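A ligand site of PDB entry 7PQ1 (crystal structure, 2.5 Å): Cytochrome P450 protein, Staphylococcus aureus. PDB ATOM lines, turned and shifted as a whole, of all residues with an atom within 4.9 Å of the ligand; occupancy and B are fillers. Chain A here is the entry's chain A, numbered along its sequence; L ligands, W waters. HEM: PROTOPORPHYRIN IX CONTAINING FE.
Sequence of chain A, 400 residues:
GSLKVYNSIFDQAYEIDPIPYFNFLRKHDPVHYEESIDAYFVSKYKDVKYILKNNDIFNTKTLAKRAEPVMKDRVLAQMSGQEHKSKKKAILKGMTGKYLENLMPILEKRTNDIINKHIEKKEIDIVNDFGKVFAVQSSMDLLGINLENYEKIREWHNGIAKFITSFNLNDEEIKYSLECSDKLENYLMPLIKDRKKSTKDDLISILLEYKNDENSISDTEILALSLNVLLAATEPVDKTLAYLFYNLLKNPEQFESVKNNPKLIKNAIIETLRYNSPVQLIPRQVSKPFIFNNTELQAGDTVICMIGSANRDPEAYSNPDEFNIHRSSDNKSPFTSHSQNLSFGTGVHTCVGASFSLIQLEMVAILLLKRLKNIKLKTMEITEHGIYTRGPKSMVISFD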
ATOM      1  N   LEU A  52     -25.678  -3.249  34.748  1.00  0.00           N
ATOM      2  CA  LEU A  52     -24.560  -4.190  34.823  1.00  0.00           C
ATOM      3  C   LEU A  52     -23.349  -3.612  35.547  1.00  0.00           C
ATOM      4  O   LEU A  52     -22.533  -4.386  36.059  1.00  0.00           O
ATOM      5  CB  LEU A  52     -24.174  -4.636  33.413  1.00  0.00           C
ATOM      6  CG  LEU A  52     -25.295  -5.240  32.559  1.00  0.00           C
ATOM      7  CD1 LEU A  52     -24.843  -5.399  31.116  1.00  0.00           C
ATOM      8  CD2 LEU A  52     -25.748  -6.573  33.124  1.00  0.00           C
ATOM      9  N   LEU A  63     -30.111 -15.640  39.007  1.00  0.00           N
ATOM     10  CA  LEU A  63     -29.416 -16.706  38.308  1.00  0.00           C
ATOM     11  C   LEU A  63     -29.134 -17.880  39.234  1.00  0.00           C
ATOM     12  O   LEU A  63     -29.282 -19.042  38.846  1.00  0.00           O
ATOM     13  CB  LEU A  63     -28.120 -16.169  37.711  1.00  0.00           C
ATOM     14  CG  LEU A  63     -28.219 -15.021  36.700  1.00  0.00           C
ATOM     15  CD1 LEU A  63     -27.950 -13.691  37.376  1.00  0.00           C
ATOM     16  CD2 LEU A  63     -27.262 -15.241  35.543  1.00  0.00           C
ATOM     17  N   LEU A  76     -20.093 -19.093  39.233  1.00  0.00           N
ATOM     18  CA  LEU A  76     -19.327 -17.849  39.364  1.00  0.00           C
ATOM     19  C   LEU A  76     -20.238 -16.640  39.568  1.00  0.00           C
ATOM     20  O   LEU A  76     -19.901 -15.725  40.335  1.00  0.00           O
ATOM     21  CB  LEU A  76     -18.458 -17.644  38.127  1.00  0.00           C
ATOM     22  CG  LEU A  76     -17.189 -16.807  38.308  1.00  0.00           C
ATOM     23  CD1 LEU A  76     -16.244 -17.494  39.286  1.00  0.00           C
ATOM     24  CD2 LEU A  76     -16.495 -16.556  36.973  1.00  0.00           C
ATOM     25  N   ALA A  77     -21.379 -16.612  38.884  1.00  0.00           N
ATOM     26  CA  ALA A  77     -22.286 -15.477  39.017  1.00  0.00           C
ATOM     27  C   ALA A  77     -22.899 -15.376  40.403  1.00  0.00           C
ATOM     28  O   ALA A  77     -23.314 -14.277  40.807  1.00  0.00           O
ATOM     29  CB  ALA A  77     -23.396 -15.562  37.960  1.00  0.00           C
ATOM     30  N   HIS A  84     -15.112 -14.430  43.995  1.00  0.00           N
ATOM     31  CA  HIS A  84     -15.407 -14.250  42.581  1.00  0.00           C
ATOM     32  C   HIS A  84     -14.154 -13.900  41.797  1.00  0.00           C
ATOM     33  O   HIS A  84     -13.906 -14.456  40.712  1.00  0.00           O
ATOM     34  CB  HIS A  84     -16.475 -13.171  42.394  1.00  0.00           C
ATOM     35  CG  HIS A  84     -16.691 -12.773  40.960  1.00  0.00           C
ATOM     36  ND1 HIS A  84     -15.972 -11.771  40.348  1.00  0.00           N
ATOM     37  CD2 HIS A  84     -17.553 -13.245  40.030  1.00  0.00           C
ATOM     38  CE1 HIS A  84     -16.380 -11.647  39.096  1.00  0.00           C
ATOM     39  NE2 HIS A  84     -17.334 -12.529  38.875  1.00  0.00           N
ATOM     40  N   LYS A  88     -12.545 -16.438  39.198  1.00  0.00           N
ATOM     41  CA  LYS A  88     -12.583 -15.931  37.829  1.00  0.00           C
ATOM     42  C   LYS A  88     -11.177 -15.904  37.227  1.00  0.00           C
ATOM     43  O   LYS A  88     -10.954 -16.412  36.114  1.00  0.00           O
ATOM     44  CB  LYS A  88     -13.202 -14.535  37.797  1.00  0.00           C
ATOM     45  CG  LYS A  88     -13.409 -13.956  36.412  1.00  0.00           C
ATOM     46  CD  LYS A  88     -14.351 -12.761  36.475  1.00  0.00           C
ATOM     47  CE  LYS A  88     -14.697 -12.244  35.095  1.00  0.00           C
ATOM     48  NZ  LYS A  88     -15.674 -11.122  35.158  1.00  0.00           N
ATOM     49  N   ILE A  91     -10.106 -19.368  36.276  1.00  0.00           N
ATOM     50  CA  ILE A  91     -10.679 -19.853  35.030  1.00  0.00           C
ATOM     51  C   ILE A  91      -9.970 -19.213  33.839  1.00  0.00           C
ATOM     52  O   ILE A  91      -9.638 -19.888  32.850  1.00  0.00           O
ATOM     53  CB  ILE A  91     -12.195 -19.599  34.991  1.00  0.00           C
ATOM     54  CG1 ILE A  91     -12.929 -20.587  35.895  1.00  0.00           C
ATOM     55  CG2 ILE A  91     -12.733 -19.683  33.567  1.00  0.00           C
ATOM     56  CD1 ILE A  91     -14.409 -20.277  36.042  1.00  0.00           C
ATOM     57  N   MET A  95      -7.454 -20.212  29.626  1.00  0.00           N
ATOM     58  CA  MET A  95      -7.540 -19.775  28.232  1.00  0.00           C
ATOM     59  C   MET A  95      -6.595 -18.611  27.951  1.00  0.00           C
ATOM     60  O   MET A  95      -6.799 -17.849  27.005  1.00  0.00           O
ATOM     61  CB  MET A  95      -8.977 -19.417  27.852  1.00  0.00           C
ATOM     62  CG  MET A  95      -9.525 -18.140  28.476  1.00  0.00           C
ATOM     63  SD  MET A  95     -11.242 -18.312  29.044  1.00  0.00           S
ATOM     64  CE  MET A  95     -11.158 -19.867  29.924  1.00  0.00           C
ATOM     65  N   LEU A 142     -10.841 -27.277  26.201  1.00  0.00           N
ATOM     66  CA  LEU A 142     -10.483 -26.286  27.207  1.00  0.00           C
ATOM     67  C   LEU A 142     -10.534 -26.881  28.613  1.00  0.00           C
ATOM     68  O   LEU A 142      -9.593 -26.721  29.392  1.00  0.00           O
ATOM     69  CB  LEU A 142     -11.418 -25.076  27.096  1.00  0.00           C
ATOM     70  CG  LEU A 142     -11.376 -24.060  28.245  1.00  0.00           C
ATOM     71  CD1 LEU A 142     -10.043 -23.334  28.281  1.00  0.00           C
ATOM     72  CD2 LEU A 142     -12.524 -23.064  28.122  1.00  0.00           C
ATOM     73  N   ASN A 228     -20.327 -24.708  34.344  1.00  0.00           N
ATOM     74  CA  ASN A 228     -20.523 -23.309  34.013  1.00  0.00           C
ATOM     75  C   ASN A 228     -19.687 -22.910  32.810  1.00  0.00           C
ATOM     76  O   ASN A 228     -20.137 -22.122  31.967  1.00  0.00           O
ATOM     77  CB  ASN A 228     -20.187 -22.433  35.219  1.00  0.00           C
ATOM     78  CG  ASN A 228     -20.482 -20.963  34.981  1.00  0.00           C
ATOM     79  OD1 ASN A 228     -21.301 -20.603  34.141  1.00  0.00           O
ATOM     80  ND2 ASN A 228     -19.810 -20.085  35.740  1.00  0.00           N
ATOM     81  N   VAL A 229     -18.475 -23.455  32.696  1.00  0.00           N
ATOM     82  CA  VAL A 229     -17.648 -23.191  31.525  1.00  0.00           C
ATOM     83  C   VAL A 229     -18.254 -23.845  30.287  1.00  0.00           C
ATOM     84  O   VAL A 229     -18.294 -23.247  29.205  1.00  0.00           O
ATOM     85  CB  VAL A 229     -16.199 -23.653  31.774  1.00  0.00           C
ATOM     86  CG1 VAL A 229     -15.422 -23.772  30.464  1.00  0.00           C
ATOM     87  CG2 VAL A 229     -15.491 -22.718  32.744  1.00  0.00           C
ATOM     88  N   ALA A 232     -21.350 -21.903  29.136  1.00  0.00           N
ATOM     89  CA  ALA A 232     -21.112 -20.511  28.744  1.00  0.00           C
ATOM     90  C   ALA A 232     -20.290 -20.404  27.469  1.00  0.00           C
ATOM     91  O   ALA A 232     -20.354 -19.384  26.781  1.00  0.00           O
ATOM     92  CB  ALA A 232     -20.427 -19.758  29.879  1.00  0.00           C
ATOM     93  N   ALA A 233     -19.527 -21.448  27.130  1.00  0.00           N
ATOM     94  CA  ALA A 233     -18.629 -21.394  25.983  1.00  0.00           C
ATOM     95  C   ALA A 233     -19.201 -22.011  24.716  1.00  0.00           C
ATOM     96  O   ALA A 233     -18.785 -21.639  23.616  1.00  0.00           O
ATOM     97  CB  ALA A 233     -17.303 -22.084  26.316  1.00  0.00           C
ATOM     98  N   PRO A 236     -22.926 -19.852  22.708  1.00  0.00           N
ATOM     99  CA  PRO A 236     -22.610 -18.558  22.067  1.00  0.00           C
ATOM    100  C   PRO A 236     -21.679 -18.668  20.868  1.00  0.00           C
ATOM    101  O   PRO A 236     -21.931 -18.021  19.841  1.00  0.00           O
ATOM    102  CB  PRO A 236     -21.966 -17.758  23.217  1.00  0.00           C
ATOM    103  CG  PRO A 236     -22.511 -18.369  24.450  1.00  0.00           C
ATOM    104  CD  PRO A 236     -22.584 -19.834  24.143  1.00  0.00           C
ATOM    105  N   VAL A 237     -20.622 -19.474  20.974  1.00  0.00           N
ATOM    106  CA  VAL A 237     -19.625 -19.529  19.911  1.00  0.00           C
ATOM    107  C   VAL A 237     -20.226 -20.089  18.619  1.00  0.00           C
ATOM    108  O   VAL A 237     -19.959 -19.587  17.527  1.00  0.00           O
ATOM    109  CB  VAL A 237     -18.399 -20.344  20.362  1.00  0.00           C
ATOM    110  CG1 VAL A 237     -17.475 -20.633  19.196  1.00  0.00           C
ATOM    111  CG2 VAL A 237     -17.644 -19.591  21.457  1.00  0.00           C
ATOM    112  N   THR A 240     -22.560 -17.362  16.868  1.00  0.00           N
ATOM    113  CA  THR A 240     -21.810 -16.230  16.341  1.00  0.00           C
ATOM    114  C   THR A 240     -21.163 -16.554  14.998  1.00  0.00           C
ATOM    115  O   THR A 240     -21.174 -15.733  14.083  1.00  0.00           O
ATOM    116  CB  THR A 240     -20.745 -15.794  17.347  1.00  0.00           C
ATOM    117  OG1 THR A 240     -21.367 -15.416  18.586  1.00  0.00           O
ATOM    118  CG2 THR A 240     -19.941 -14.611  16.813  1.00  0.00           C
ATOM    119  N   LEU A 273     -21.171  -9.501  16.638  1.00  0.00           N
ATOM    120  CA  LEU A 273     -21.644  -9.681  18.005  1.00  0.00           C
ATOM    121  C   LEU A 273     -22.580  -8.558  18.424  1.00  0.00           C
ATOM    122  O   LEU A 273     -23.537  -8.781  19.182  1.00  0.00           O
ATOM    123  CB  LEU A 273     -20.444  -9.766  18.950  1.00  0.00           C
ATOM    124  CG  LEU A 273     -19.702 -11.102  18.905  1.00  0.00           C
ATOM    125  CD1 LEU A 273     -18.384 -11.039  19.667  1.00  0.00           C
ATOM    126  CD2 LEU A 273     -20.587 -12.207  19.449  1.00  0.00           C
ATOM    127  N   PRO A 278     -25.699 -12.946  20.313  1.00  0.00           N
ATOM    128  CA  PRO A 278     -26.139 -14.332  20.533  1.00  0.00           C
ATOM    129  C   PRO A 278     -26.711 -14.539  21.920  1.00  0.00           C
ATOM    130  O   PRO A 278     -27.693 -15.287  22.083  1.00  0.00           O
ATOM    131  CB  PRO A 278     -24.869 -15.150  20.293  1.00  0.00           C
ATOM    132  CG  PRO A 278     -23.732 -14.194  20.297  1.00  0.00           C
ATOM    133  CD  PRO A 278     -24.237 -12.788  20.308  1.00  0.00           C
ATOM    134  N   VAL A 279     -26.134 -13.897  22.926  1.00  0.00           N
ATOM    135  CA  VAL A 279     -26.713 -13.856  24.267  1.00  0.00           C
ATOM    136  C   VAL A 279     -27.589 -12.621  24.332  1.00  0.00           C
ATOM    137  O   VAL A 279     -27.098 -11.492  24.338  1.00  0.00           O
ATOM    138  CB  VAL A 279     -25.630 -13.826  25.346  1.00  0.00           C
ATOM    139  CG1 VAL A 279     -26.251 -13.594  26.717  1.00  0.00           C
ATOM    140  CG2 VAL A 279     -24.823 -15.124  25.336  1.00  0.00           C
ATOM    141  N   ILE A 282     -29.868 -10.870  30.008  1.00  0.00           N
ATOM    142  CA  ILE A 282     -29.081 -11.004  31.231  1.00  0.00           C
ATOM    143  C   ILE A 282     -29.943 -10.569  32.418  1.00  0.00           C
ATOM    144  O   ILE A 282     -30.233  -9.372  32.569  1.00  0.00           O
ATOM    145  CB  ILE A 282     -27.785 -10.175  31.173  1.00  0.00           C
ATOM    146  CG1 ILE A 282     -26.881 -10.619  30.026  1.00  0.00           C
ATOM    147  CG2 ILE A 282     -27.027 -10.253  32.487  1.00  0.00           C
ATOM    148  CD1 ILE A 282     -25.676  -9.732  29.873  1.00  0.00           C
ATOM    149  N   ARG A 284     -31.153  -9.752  36.381  1.00  0.00           N
ATOM    150  CA  ARG A 284     -30.607  -9.191  37.614  1.00  0.00           C
ATOM    151  C   ARG A 284     -31.756  -8.996  38.598  1.00  0.00           C
ATOM    152  O   ARG A 284     -32.924  -8.914  38.210  1.00  0.00           O
ATOM    153  CB  ARG A 284     -29.887  -7.859  37.365  1.00  0.00           C
ATOM    154  CG  ARG A 284     -28.527  -7.992  36.682  1.00  0.00           C
ATOM    155  CD  ARG A 284     -27.520  -8.747  37.548  1.00  0.00           C
ATOM    156  NE  ARG A 284     -26.157  -8.677  37.027  1.00  0.00           N
ATOM    157  CZ  ARG A 284     -25.653  -9.536  36.158  1.00  0.00           C
ATOM    158  NH1 ARG A 284     -26.354 -10.559  35.696  1.00  0.00           N
ATOM    159  NH2 ARG A 284     -24.399  -9.382  35.745  1.00  0.00           N
ATOM    160  N   LEU A 342     -22.303  -4.357  24.346  1.00  0.00           N
ATOM    161  CA  LEU A 342     -22.485  -5.142  25.566  1.00  0.00           C
ATOM    162  C   LEU A 342     -22.697  -6.620  25.254  1.00  0.00           C
ATOM    163  O   LEU A 342     -23.319  -7.339  26.046  1.00  0.00           O
ATOM    164  CB  LEU A 342     -23.659  -4.588  26.383  1.00  0.00           C
ATOM    165  CG  LEU A 342     -23.638  -3.083  26.652  1.00  0.00           C
ATOM    166  CD1 LEU A 342     -25.063  -2.539  26.715  1.00  0.00           C
ATOM    167  CD2 LEU A 342     -22.903  -2.766  27.944  1.00  0.00           C
ATOM    168  N   SER A 343     -22.177  -7.098  24.124  1.00  0.00           N
ATOM    169  CA  SER A 343     -22.321  -8.515  23.767  1.00  0.00           C
ATOM    170  C   SER A 343     -21.721  -9.418  24.851  1.00  0.00           C
ATOM    171  O   SER A 343     -22.247 -10.507  25.109  1.00  0.00           O
ATOM    172  CB  SER A 343     -21.679  -8.801  22.409  1.00  0.00           C
ATOM    173  OG  SER A 343     -22.340  -9.855  21.722  1.00  0.00           O
ATOM    174  N   PHE A 344     -20.635  -8.984  25.483  1.00  0.00           N
ATOM    175  CA  PHE A 344     -20.046  -9.697  26.603  1.00  0.00           C
ATOM    176  C   PHE A 344     -20.464  -9.121  27.945  1.00  0.00           C
ATOM    177  O   PHE A 344     -19.766  -9.308  28.947  1.00  0.00           O
ATOM    178  CB  PHE A 344     -18.514  -9.686  26.494  1.00  0.00           C
ATOM    179  CG  PHE A 344     -18.000 -10.341  25.249  1.00  0.00           C
ATOM    180  CD1 PHE A 344     -17.906 -11.720  25.164  1.00  0.00           C
ATOM    181  CD2 PHE A 344     -17.609  -9.577  24.160  1.00  0.00           C
ATOM    182  CE1 PHE A 344     -17.424 -12.328  24.027  1.00  0.00           C
ATOM    183  CE2 PHE A 344     -17.129 -10.172  23.018  1.00  0.00           C
ATOM    184  CZ  PHE A 344     -17.039 -11.560  22.950  1.00  0.00           C
ATOM    185  N   GLY A 345     -21.596  -8.422  27.997  1.00  0.00           N
ATOM    186  CA  GLY A 345     -21.985  -7.752  29.222  1.00  0.00           C
ATOM    187  C   GLY A 345     -20.934  -6.700  29.587  1.00  0.00           C
ATOM    188  O   GLY A 345     -20.170  -6.226  28.749  1.00  0.00           O
ATOM    189  N   VAL A 348     -18.844  -6.331  36.789  1.00  0.00           N
ATOM    190  CA  VAL A 348     -18.120  -7.349  37.545  1.00  0.00           C
ATOM    191  C   VAL A 348     -18.226  -8.699  36.863  1.00  0.00           C
ATOM    192  O   VAL A 348     -17.218  -9.394  36.670  1.00  0.00           O
ATOM    193  CB  VAL A 348     -18.629  -7.392  38.996  1.00  0.00           C
ATOM    194  CG1 VAL A 348     -18.242  -8.704  39.659  1.00  0.00           C
ATOM    195  CG2 VAL A 348     -18.100  -6.205  39.787  1.00  0.00           C
ATOM    196  N   HIS A 349     -19.438  -9.103  36.481  1.00  0.00           N
ATOM    197  CA  HIS A 349     -19.678 -10.407  35.883  1.00  0.00           C
ATOM    198  C   HIS A 349     -19.521 -10.395  34.365  1.00  0.00           C
ATOM    199  O   HIS A 349     -20.200 -11.173  33.667  1.00  0.00           O
ATOM    200  CB  HIS A 349     -21.063 -10.916  36.290  1.00  0.00           C
ATOM    201  CG  HIS A 349     -21.200 -11.167  37.759  1.00  0.00           C
ATOM    202  ND1 HIS A 349     -20.687 -12.280  38.382  1.00  0.00           N
ATOM    203  CD2 HIS A 349     -21.781 -10.420  38.736  1.00  0.00           C
ATOM    204  CE1 HIS A 349     -20.954 -12.225  39.678  1.00  0.00           C
ATOM    205  NE2 HIS A 349     -21.620 -11.110  39.916  1.00  0.00           N
ATOM    206  N   THR A 350     -18.642  -9.551  33.825  1.00  0.00           N
ATOM    207  CA  THR A 350     -18.404  -9.549  32.390  1.00  0.00           C
ATOM    208  C   THR A 350     -17.653 -10.814  31.981  1.00  0.00           C
ATOM    209  O   THR A 350     -16.928 -11.417  32.777  1.00  0.00           O
ATOM    210  CB  THR A 350     -17.601  -8.306  31.989  1.00  0.00           C
ATOM    211  OG1 THR A 350     -17.308  -8.353  30.589  1.00  0.00           O
ATOM    212  CG2 THR A 350     -16.282  -8.256  32.756  1.00  0.00           C
ATOM    213  N   CYS A 351     -17.838 -11.209  30.724  1.00  0.00           N
ATOM    214  CA  CYS A 351     -17.426 -12.543  30.268  1.00  0.00           C
ATOM    215  C   CYS A 351     -15.926 -12.750  30.430  1.00  0.00           C
ATOM    216  O   CYS A 351     -15.121 -11.993  29.884  1.00  0.00           O
ATOM    217  CB  CYS A 351     -17.840 -12.743  28.803  1.00  0.00           C
ATOM    218  SG  CYS A 351     -17.428 -14.371  28.127  1.00  0.00           S
ATOM    219  N   VAL A 352     -15.558 -13.807  31.161  1.00  0.00           N
ATOM    220  CA  VAL A 352     -14.160 -14.145  31.335  1.00  0.00           C
ATOM    221  C   VAL A 352     -13.562 -14.673  30.038  1.00  0.00           C
ATOM    222  O   VAL A 352     -12.355 -14.554  29.802  1.00  0.00           O
ATOM    223  CB  VAL A 352     -13.991 -15.149  32.493  1.00  0.00           C
ATOM    224  CG1 VAL A 352     -14.478 -16.544  32.088  1.00  0.00           C
ATOM    225  CG2 VAL A 352     -12.547 -15.212  32.957  1.00  0.00           C
ATOM    226  N   GLY A 353     -14.384 -15.241  29.159  1.00  0.00           N
ATOM    227  CA  GLY A 353     -13.882 -15.838  27.930  1.00  0.00           C
ATOM    228  C   GLY A 353     -14.009 -14.929  26.733  1.00  0.00           C
ATOM    229  O   GLY A 353     -14.119 -15.397  25.595  1.00  0.00           O
ATOM    230  N   PHE A 356     -10.673 -14.914  24.647  1.00  0.00           N
ATOM    231  CA  PHE A 356     -10.528 -16.249  24.080  1.00  0.00           C
ATOM    232  C   PHE A 356     -11.557 -16.494  22.985  1.00  0.00           C
ATOM    233  O   PHE A 356     -11.256 -17.154  21.984  1.00  0.00           O
ATOM    234  CB  PHE A 356     -10.653 -17.292  25.194  1.00  0.00           C
ATOM    235  CG  PHE A 356     -10.717 -18.705  24.709  1.00  0.00           C
ATOM    236  CD1 PHE A 356      -9.692 -19.228  23.941  1.00  0.00           C
ATOM    237  CD2 PHE A 356     -11.788 -19.508  25.029  1.00  0.00           C
ATOM    238  CE1 PHE A 356      -9.744 -20.533  23.492  1.00  0.00           C
ATOM    239  CE2 PHE A 356     -11.842 -20.818  24.588  1.00  0.00           C
ATOM    240  CZ  PHE A 356     -10.821 -21.332  23.824  1.00  0.00           C
ATOM    241  N   SER A 357     -12.782 -15.975  23.151  1.00  0.00           N
ATOM    242  CA  SER A 357     -13.799 -16.147  22.119  1.00  0.00           C
ATOM    243  C   SER A 357     -13.424 -15.416  20.837  1.00  0.00           C
ATOM    244  O   SER A 357     -13.607 -15.954  19.737  1.00  0.00           O
ATOM    245  CB  SER A 357     -15.156 -15.662  22.626  1.00  0.00           C
ATOM    246  OG  SER A 357     -15.680 -16.570  23.587  1.00  0.00           O
ATOM    247  N   LEU A 361     -12.562 -17.443  17.447  1.00  0.00           N
ATOM    248  CA  LEU A 361     -13.443 -17.197  16.304  1.00  0.00           C
ATOM    249  C   LEU A 361     -12.680 -16.655  15.099  1.00  0.00           C
ATOM    250  O   LEU A 361     -13.089 -16.879  13.957  1.00  0.00           O
ATOM    251  CB  LEU A 361     -14.573 -16.249  16.690  1.00  0.00           C
ATOM    252  CG  LEU A 361     -15.693 -16.848  17.539  1.00  0.00           C
ATOM    253  CD1 LEU A 361     -16.511 -15.758  18.221  1.00  0.00           C
ATOM    254  CD2 LEU A 361     -16.583 -17.740  16.697  1.00  0.00           C
HETATM  255  CHA HEM L   1     -20.260 -14.241  31.338  1.00  0.00           C
HETATM  256  CHB HEM L   1     -21.470 -13.736  26.666  1.00  0.00           C
HETATM  257  CHC HEM L   1     -18.033 -16.920  25.427  1.00  0.00           C
HETATM  258  CHD HEM L   1     -17.506 -18.068  30.123  1.00  0.00           C
HETATM  259  C1A HEM L   1     -20.869 -13.767  30.182  1.00  0.00           C
HETATM  260  C2A HEM L   1     -21.836 -12.689  30.076  1.00  0.00           C
HETATM  261  C3A HEM L   1     -22.160 -12.571  28.784  1.00  0.00           C
HETATM  262  C4A HEM L   1     -21.413 -13.545  28.029  1.00  0.00           C
HETATM  263  CMA HEM L   1     -23.160 -11.558  28.177  1.00  0.00           C
HETATM  264  CAA HEM L   1     -22.410 -11.848  31.230  1.00  0.00           C
HETATM  265  CBA HEM L   1     -23.356 -12.704  32.069  1.00  0.00           C
HETATM  266  CGA HEM L   1     -23.924 -11.900  33.205  1.00  0.00           C
HETATM  267  O1A HEM L   1     -24.619 -12.494  34.067  1.00  0.00           O
HETATM  268  O2A HEM L   1     -23.684 -10.673  33.247  1.00  0.00           O
HETATM  269  C1B HEM L   1     -20.598 -14.498  25.923  1.00  0.00           C
HETATM  270  C2B HEM L   1     -20.467 -14.460  24.481  1.00  0.00           C
HETATM  271  C3B HEM L   1     -19.519 -15.344  24.119  1.00  0.00           C
HETATM  272  C4B HEM L   1     -19.017 -15.960  25.337  1.00  0.00           C
HETATM  273  CMB HEM L   1     -21.327 -13.527  23.592  1.00  0.00           C
HETATM  274  CAB HEM L   1     -18.965 -15.716  22.707  1.00  0.00           C
HETATM  275  CBB HEM L   1     -19.231 -15.048  21.584  1.00  0.00           C
HETATM  276  C1C HEM L   1     -17.559 -17.510  26.583  1.00  0.00           C
HETATM  277  C2C HEM L   1     -16.473 -18.471  26.697  1.00  0.00           C
HETATM  278  C3C HEM L   1     -16.323 -18.790  27.983  1.00  0.00           C
HETATM  279  C4C HEM L   1     -17.312 -18.045  28.758  1.00  0.00           C
HETATM  280  CMC HEM L   1     -15.627 -19.038  25.531  1.00  0.00           C
HETATM  281  CAC HEM L   1     -15.265 -19.795  28.492  1.00  0.00           C
HETATM  282  CBC HEM L   1     -15.167 -20.160  29.776  1.00  0.00           C
HETATM  283  C1D HEM L   1     -18.193 -17.131  30.862  1.00  0.00           C
HETATM  284  C2D HEM L   1     -18.274 -17.065  32.301  1.00  0.00           C
HETATM  285  C3D HEM L   1     -19.034 -16.017  32.631  1.00  0.00           C
HETATM  286  C4D HEM L   1     -19.457 -15.367  31.414  1.00  0.00           C
HETATM  287  CMD HEM L   1     -17.608 -18.042  33.293  1.00  0.00           C
HETATM  288  CAD HEM L   1     -19.376 -15.563  34.067  1.00  0.00           C
HETATM  289  CBD HEM L   1     -18.537 -14.329  34.359  1.00  0.00           C
HETATM  290  CGD HEM L   1     -18.743 -13.853  35.770  1.00  0.00           C
HETATM  291  O1D HEM L   1     -19.792 -14.185  36.383  1.00  0.00           O
HETATM  292  O2D HEM L   1     -17.852 -13.120  36.290  1.00  0.00           O
HETATM  293  NA  HEM L   1     -20.633 -14.266  28.916  1.00  0.00           N
HETATM  294  NB  HEM L   1     -19.696 -15.420  26.403  1.00  0.00           N
HETATM  295  NC  HEM L   1     -18.036 -17.273  27.864  1.00  0.00           N
HETATM  296  ND  HEM L   1     -18.934 -16.070  30.354  1.00  0.00           N
HETATM  297 FE   HEM L   1     -19.264 -15.712  28.379  1.00  0.00          FE
HETATM  298  O   HOH W   1     -22.034  -8.211  32.811  1.00  0.00           O
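The side-chain hydroxyl of Thr 350 is in hydrogen-bond range of the backbone carbonyl oxygen of Phe 344 (3.1 Å).
O of Thr 350 sits at hydrogen-bond distance from NZ of Lys 88, 2.7 Å away.
N of Gly 353 sits close to SG of Cys 351 (3.3 Å).
The side-chain hydroxyl (OG) of Ser 357 sits at hydrogen-bond distance from the backbone carbonyl oxygen (O) of Gly 353, 2.8 Å away.
OG1 of Thr 240 lies within hydrogen-bond range of O of Pro 236, at 2.9 Å.
A ring nitrogen (NE2) of His 84 sits at hydrogen-bond distance from a ring nitrogen (ND1) of His 349 (3.4 Å).
N of Cys 351 lies within hydrogen-bond range of O of Phe 344.
O of Leu 273 is in hydrogen-bond range of OG of Ser 343 (3.0 Å).
A ring nitrogen (ND1) of His 349 lies within hydrogen-bond range of an oxygen (O1D) of the ligand, at 2.9 Å.
O2D of the ligand is in hydrogen-bond range of NE2 of His 84 (2.7 Å).
An oxygen (O2D) of the ligand lies within salt-bridge range of the side-chain amino group of Lys 88.
The guanidinium group (NH2) of Arg 284 lies within salt-bridge range of an oxygen (O2A) of the ligand, 2.9 Å away.
FE of the ligand is bound by SG of Cys 351 (2.3 Å).
A nitrogen (NC) of the ligand sits close to the backbone carbonyl oxygen (O) of Ala 232 (3.3 Å).
Leu 76 touches the ligand (CD2 to CGD, 3.7 Å).
Ala 77 touches the ligand (N to O1D, 3.8 Å).
ND2 of Asn 228 touches CMD of the ligand, 3.9 Å away.
CG1 of Val 229 touches CBC of the ligand (3.7 Å).
CB of Ala 233 touches CMC of the ligand, at 3.6 Å.
Pro 236 touches the ligand (CB to C3B, 3.6 Å).
OG1 of Thr 240 touches CBB of the ligand, 3.7 Å away.
Leu 273 touches the ligand (CD2 to CBB, 3.8 Å).
CG2 of Val 279 touches CHB of the ligand, 3.9 Å away.
Ile 282 touches the ligand.
Ser 343 touches the ligand (O to CMA, 3.4 Å).
Phe 344 touches the ligand.
Gly 345 touches the ligand (N to CMA, 3.5 Å).
Val 348 touches the ligand.
O of Thr 350 touches CBD of the ligand, at 3.7 Å.
CG1 of Val 352 touches CMD of the ligand (3.7 Å).
CA of Gly 353 touches C3C of the ligand, 3.8 Å away.
Phe 356 touches the ligand.
OG of Ser 357 touches CHC of the ligand (3.0 Å).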
